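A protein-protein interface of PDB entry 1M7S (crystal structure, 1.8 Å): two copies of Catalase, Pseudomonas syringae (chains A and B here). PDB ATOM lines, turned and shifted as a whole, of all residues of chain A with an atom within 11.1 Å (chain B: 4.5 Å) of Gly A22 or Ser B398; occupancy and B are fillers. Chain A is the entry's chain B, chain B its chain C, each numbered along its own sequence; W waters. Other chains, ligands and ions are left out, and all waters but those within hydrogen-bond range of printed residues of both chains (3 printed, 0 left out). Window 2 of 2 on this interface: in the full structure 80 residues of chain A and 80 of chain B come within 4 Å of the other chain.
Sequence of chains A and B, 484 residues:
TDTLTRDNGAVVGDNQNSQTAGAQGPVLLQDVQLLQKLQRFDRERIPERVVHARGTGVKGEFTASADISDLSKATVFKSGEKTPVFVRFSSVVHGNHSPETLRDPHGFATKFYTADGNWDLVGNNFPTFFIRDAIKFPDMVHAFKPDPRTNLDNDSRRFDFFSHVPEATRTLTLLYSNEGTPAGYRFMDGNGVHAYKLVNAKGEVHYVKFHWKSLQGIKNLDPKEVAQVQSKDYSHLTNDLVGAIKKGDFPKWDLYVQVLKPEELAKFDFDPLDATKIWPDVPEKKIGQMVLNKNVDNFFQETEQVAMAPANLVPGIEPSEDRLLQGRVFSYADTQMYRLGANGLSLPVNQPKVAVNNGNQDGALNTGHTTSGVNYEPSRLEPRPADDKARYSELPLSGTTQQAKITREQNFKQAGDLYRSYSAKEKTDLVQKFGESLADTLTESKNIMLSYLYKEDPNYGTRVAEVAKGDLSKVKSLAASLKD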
ATOM      1  N   ASN A  17     -10.252  12.051   7.562  1.00  0.00           N
ATOM      2  CA  ASN A  17      -9.681  10.734   7.652  1.00  0.00           C
ATOM      3  C   ASN A  17      -8.159  10.709   7.870  1.00  0.00           C
ATOM      4  O   ASN A  17      -7.473  11.416   7.125  1.00  0.00           O
ATOM      5  CB  ASN A  17      -9.916   9.960   6.333  1.00  0.00           C
ATOM      6  CG  ASN A  17     -11.440   9.917   6.074  1.00  0.00           C
ATOM      7  OD1 ASN A  17     -12.163   9.329   6.864  1.00  0.00           O
ATOM      8  ND2 ASN A  17     -11.886  10.591   5.031  1.00  0.00           N
ATOM      9  N   SER A  18      -7.738   9.890   8.827  1.00  0.00           N
ATOM     10  CA  SER A  18      -6.287   9.685   8.993  1.00  0.00           C
ATOM     11  C   SER A  18      -5.778   8.862   7.806  1.00  0.00           C
ATOM     12  O   SER A  18      -6.525   8.106   7.162  1.00  0.00           O
ATOM     13  CB  SER A  18      -6.026   8.885  10.290  1.00  0.00           C
ATOM     14  OG  SER A  18      -6.365   9.703  11.445  1.00  0.00           O
ATOM     15  N   GLN A  19      -4.480   8.957   7.505  1.00  0.00           N
ATOM     16  CA  GLN A  19      -3.908   8.154   6.403  1.00  0.00           C
ATOM     17  C   GLN A  19      -3.634   6.758   6.937  1.00  0.00           C
ATOM     18  O   GLN A  19      -3.005   6.662   8.000  1.00  0.00           O
ATOM     19  CB  GLN A  19      -2.603   8.800   5.894  1.00  0.00           C
ATOM     20  CG  GLN A  19      -2.073   8.046   4.672  1.00  0.00           C
ATOM     21  CD  GLN A  19      -0.811   8.706   4.127  1.00  0.00           C
ATOM     22  OE1 GLN A  19      -0.067   9.335   4.904  1.00  0.00           O
ATOM     23  NE2 GLN A  19      -0.628   8.588   2.828  1.00  0.00           N
ATOM     24  N   THR A  20      -4.187   5.712   6.284  1.00  0.00           N
ATOM     25  CA  THR A  20      -4.052   4.364   6.819  1.00  0.00           C
ATOM     26  C   THR A  20      -3.438   3.435   5.762  1.00  0.00           C
ATOM     27  O   THR A  20      -3.438   3.761   4.588  1.00  0.00           O
ATOM     28  CB  THR A  20      -5.412   3.759   7.263  1.00  0.00           C
ATOM     29  OG1 THR A  20      -6.324   3.646   6.145  1.00  0.00           O
ATOM     30  CG2 THR A  20      -6.135   4.610   8.297  1.00  0.00           C
ATOM     31  N   ALA A  21      -2.938   2.280   6.200  1.00  0.00           N
ATOM     32  CA  ALA A  21      -2.321   1.318   5.276  1.00  0.00           C
ATOM     33  C   ALA A  21      -3.459   0.382   4.791  1.00  0.00           C
ATOM     34  O   ALA A  21      -3.532  -0.745   5.247  1.00  0.00           O
ATOM     35  CB  ALA A  21      -1.265   0.486   5.977  1.00  0.00           C
ATOM     36  N   GLY A  22      -4.165   0.847   3.770  1.00  0.00           N
ATOM     37  CA  GLY A  22      -5.311   0.105   3.267  1.00  0.00           C
ATOM     38  C   GLY A  22      -6.530   0.428   4.139  1.00  0.00           C
ATOM     39  O   GLY A  22      -6.480   0.864   5.307  1.00  0.00           O
ATOM     40  N   ALA A  23      -7.712   0.072   3.633  1.00  0.00           N
ATOM     41  CA  ALA A  23      -8.964   0.327   4.348  1.00  0.00           C
ATOM     42  C   ALA A  23      -9.055  -0.310   5.706  1.00  0.00           C
ATOM     43  O   ALA A  23      -9.748   0.219   6.592  1.00  0.00           O
ATOM     44  CB  ALA A  23     -10.135  -0.211   3.493  1.00  0.00           C
ATOM     45  N   GLN A  24      -8.463  -1.469   5.932  1.00  0.00           N
ATOM     46  CA  GLN A  24      -8.510  -2.136   7.220  1.00  0.00           C
ATOM     47  C   GLN A  24      -7.189  -2.093   7.969  1.00  0.00           C
ATOM     48  O   GLN A  24      -7.027  -2.813   8.951  1.00  0.00           O
ATOM     49  CB  GLN A  24      -8.935  -3.608   6.995  1.00  0.00           C
ATOM     50  CG  GLN A  24     -10.465  -3.649   6.936  1.00  0.00           C
ATOM     51  CD  GLN A  24     -10.991  -3.254   5.579  1.00  0.00           C
ATOM     52  OE1 GLN A  24     -10.471  -3.704   4.558  1.00  0.00           O
ATOM     53  NE2 GLN A  24     -12.013  -2.391   5.593  1.00  0.00           N
ATOM     54  N   GLY A  25      -6.285  -1.231   7.500  1.00  0.00           N
ATOM     55  CA  GLY A  25      -4.941  -1.213   8.064  1.00  0.00           C
ATOM     56  C   GLY A  25      -4.709  -0.106   9.083  1.00  0.00           C
ATOM     57  O   GLY A  25      -5.540   0.790   9.242  1.00  0.00           O
ATOM     58  N   PRO A  26      -3.568  -0.179   9.744  1.00  0.00           N
ATOM     59  CA  PRO A  26      -3.124   0.776  10.735  1.00  0.00           C
ATOM     60  C   PRO A  26      -2.839   2.170  10.199  1.00  0.00           C
ATOM     61  O   PRO A  26      -2.630   2.401   9.009  1.00  0.00           O
ATOM     62  CB  PRO A  26      -1.839   0.188  11.366  1.00  0.00           C
ATOM     63  CG  PRO A  26      -1.394  -0.807  10.318  1.00  0.00           C
ATOM     64  CD  PRO A  26      -2.591  -1.260   9.509  1.00  0.00           C
ATOM     65  N   VAL A  27      -2.772   3.151  11.136  1.00  0.00           N
ATOM     66  CA  VAL A  27      -2.491   4.539  10.737  1.00  0.00           C
ATOM     67  C   VAL A  27      -0.993   4.765  10.521  1.00  0.00           C
ATOM     68  O   VAL A  27      -0.146   4.217  11.198  1.00  0.00           O
ATOM     69  CB  VAL A  27      -3.014   5.492  11.836  1.00  0.00           C
ATOM     70  CG1 VAL A  27      -2.538   6.928  11.743  1.00  0.00           C
ATOM     71  CG2 VAL A  27      -4.564   5.475  11.710  1.00  0.00           C
ATOM     72  N   LEU A  28      -0.652   5.669   9.580  1.00  0.00           N
ATOM     73  CA  LEU A  28       0.741   5.896   9.253  1.00  0.00           C
ATOM     74  C   LEU A  28       1.396   7.003  10.079  1.00  0.00           C
ATOM     75  O   LEU A  28       0.787   8.050  10.221  1.00  0.00           O
ATOM     76  CB  LEU A  28       0.848   6.359   7.796  1.00  0.00           C
ATOM     77  CG  LEU A  28       0.362   5.286   6.769  1.00  0.00           C
ATOM     78  CD1 LEU A  28       0.772   5.756   5.395  1.00  0.00           C
ATOM     79  CD2 LEU A  28       0.957   3.940   7.115  1.00  0.00           C
ATOM     80  N   LEU B 397      -1.889  -7.147   4.814  1.00  0.00           N
ATOM     81  CA  LEU B 397      -2.306  -5.871   4.236  1.00  0.00           C
ATOM     82  C   LEU B 397      -2.719  -5.941   2.774  1.00  0.00           C
ATOM     83  O   LEU B 397      -2.292  -6.849   2.044  1.00  0.00           O
ATOM     84  CB  LEU B 397      -1.102  -4.895   4.267  1.00  0.00           C
ATOM     85  CG  LEU B 397      -0.547  -4.606   5.655  1.00  0.00           C
ATOM     86  CD1 LEU B 397       0.815  -3.937   5.585  1.00  0.00           C
ATOM     87  CD2 LEU B 397      -1.509  -3.693   6.430  1.00  0.00           C
ATOM     88  N   SER B 398      -3.468  -4.937   2.313  1.00  0.00           N
ATOM     89  CA  SER B 398      -3.828  -4.917   0.899  1.00  0.00           C
ATOM     90  C   SER B 398      -4.284  -3.512   0.543  1.00  0.00           C
ATOM     91  O   SER B 398      -4.363  -2.679   1.447  1.00  0.00           O
ATOM     92  CB  SER B 398      -4.963  -5.930   0.635  1.00  0.00           C
ATOM     93  OG  SER B 398      -6.227  -5.469   1.094  1.00  0.00           O
ATOM     94  N   GLY B 399      -4.532  -3.232  -0.712  1.00  0.00           N
ATOM     95  CA  GLY B 399      -5.015  -1.917  -1.141  1.00  0.00           C
ATOM     96  C   GLY B 399      -3.824  -0.969  -1.214  1.00  0.00           C
ATOM     97  O   GLY B 399      -2.728  -1.367  -1.607  1.00  0.00           O
ATOM     98  N   THR B 400      -4.057   0.271  -0.759  1.00  0.00           N
ATOM     99  CA  THR B 400      -3.023   1.295  -0.851  1.00  0.00           C
ATOM    100  C   THR B 400      -3.077   2.209   0.380  1.00  0.00           C
ATOM    101  O   THR B 400      -4.050   2.145   1.120  1.00  0.00           O
ATOM    102  CB  THR B 400      -3.248   2.272  -2.019  1.00  0.00           C
ATOM    103  OG1 THR B 400      -4.433   3.080  -1.784  1.00  0.00           O
ATOM    104  CG2 THR B 400      -3.452   1.621  -3.371  1.00  0.00           C
ATOM    105  N   THR B 401      -2.027   3.039   0.547  1.00  0.00           N
ATOM    106  CA  THR B 401      -2.123   4.038   1.609  1.00  0.00           C
ATOM    107  C   THR B 401      -3.281   4.922   1.162  1.00  0.00           C
ATOM    108  O   THR B 401      -3.480   5.172  -0.057  1.00  0.00           O
ATOM    109  CB  THR B 401      -0.800   4.786   1.840  1.00  0.00           C
ATOM    110  OG1 THR B 401      -0.409   5.385   0.622  1.00  0.00           O
ATOM    111  CG2 THR B 401       0.301   3.823   2.277  1.00  0.00           C
ATOM    112  N   GLN B 402      -4.106   5.334   2.137  1.00  0.00           N
ATOM    113  CA  GLN B 402      -5.306   6.048   1.729  1.00  0.00           C
ATOM    114  C   GLN B 402      -5.854   6.965   2.806  1.00  0.00           C
ATOM    115  O   GLN B 402      -5.468   6.811   3.944  1.00  0.00           O
ATOM    116  CB  GLN B 402      -6.385   4.941   1.471  1.00  0.00           C
ATOM    117  CG  GLN B 402      -6.750   4.114   2.668  1.00  0.00           C
ATOM    118  CD  GLN B 402      -8.144   3.505   2.661  1.00  0.00           C
ATOM    119  OE1 GLN B 402      -8.967   3.708   3.565  1.00  0.00           O
ATOM    120  NE2 GLN B 402      -8.393   2.707   1.640  1.00  0.00           N
HETATM  121  O   HOH W   1      -8.161   6.103   5.554  1.00  0.00           O
HETATM  122  O   HOH W   2      -2.888   8.240   1.045  1.00  0.00           O
HETATM  123  O   HOH W   3      -4.596  -3.395   4.689  1.00  0.00           O
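Gly A22 touches just these residues of chain B: Ser B398, Thr B400 and Gln B402.
Of chain A, only Gly A22 (3.5 Å) comes within 4 Å of Ser B398.
Of chain A, only Ala A21 (3.8 Å) comes within 4 Å of Leu B397.
No residue of chain A comes within 4 Å of Gly B399.
Of chain A, only Thr A20 (3.9 Å) and Gly A22 (3.0 Å) come within 4 Å of Thr B400.
Of chain A, only Gln A19 (3.9 Å), Thr A20 (3.3 Å) and Leu A28 (3.7 Å) come within 4 Å of Thr B401.
Gln B402 touches just these residues of chain A: Ser A18 (3.6 Å), Gln A19 (3.2 Å), Thr A20 (2.9 Å), Gly A22 (3.8 Å) and Ala A23 (3.4 Å).
Of the printed residues of chain B, Leu A28 touches Thr B401.
Of the printed residues of chain B, Gln A19 touches Thr B401 (3.9 Å) and Gln B402 (3.2 Å).
The nearest residue of chain B that does not touch Gly A22 is Thr B401 (4.4 Å).
The nearest residue of chain A that does not touch Ser B398 is Ala A21 (4.3 Å).
The nearest printed residue of chain B that does not touch Thr A20 is Ser B398 (7.2 Å).
N of Ala A23 lies close to NE2 of Gln B402, 3.4 Å away.
The backbone carbonyl oxygen (O) of Thr B400 sits at hydrogen-bond distance from the backbone NH (N) of Gly A22 (3.0 Å).
O of Gln B402 sits at hydrogen-bond distance from N of Thr A20 (2.9 Å).
Of the 12 printed residues of chain A, 7 touch a printed residue of chain B.
Hydrophobic or aromatic side chains of chain A within 4 Å of the printed part of chain B: Ala A23 and Leu A28.
Among the printed residues, 12 pairs touch across the chains.
Among the printed residues, no Asp or Glu carboxylate lies within 4 Å of a Lys or Arg side-chain nitrogen of the other chain.
Water W2 lies within hydrogen-bond range of NE2 of Gln A19 (2.9 Å), O of Thr B401 (3.3 Å) and N of Gln B402 (3.3 Å).
Water W3 lies within hydrogen-bond range of the backbone carbonyl oxygen of Ala A21 and the backbone NH of Ser B398.
Water W1 lies within hydrogen-bond range of the backbone carbonyl oxygen of Ser A18 (3.0 Å), the side-chain hydroxyl of Thr A20 (3.1 Å) and the backbone carbonyl oxygen of Gln B402 (3.2 Å).
Among the printed residues, pairs that only touch across the chains: Gln A19 with Gln B402, Thr A20 with Thr B401, Gly A22 with Ser B398, Ser A18 with Gln B402, Leu A28 with Thr B401, Ala A21 with Leu B397, Gly A22 with Gln B402, Thr A20 with Thr B400 and Gln A19 with Thr B401.
No position is printed for both chains.
The backbone NH of Ala A21 sits at hydrogen-bond distance from the backbone carbonyl oxygen of Pro A26 (2.8 Å).
The side-chain hydroxyl (OG1) of Thr A20 lies within hydrogen-bond range of the backbone carbonyl oxygen (O) of Gly A22, at 2.9 Å.
The backbone NH of Leu A28 is in hydrogen-bond range of the backbone carbonyl oxygen of Gln A19 (3.0 Å).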
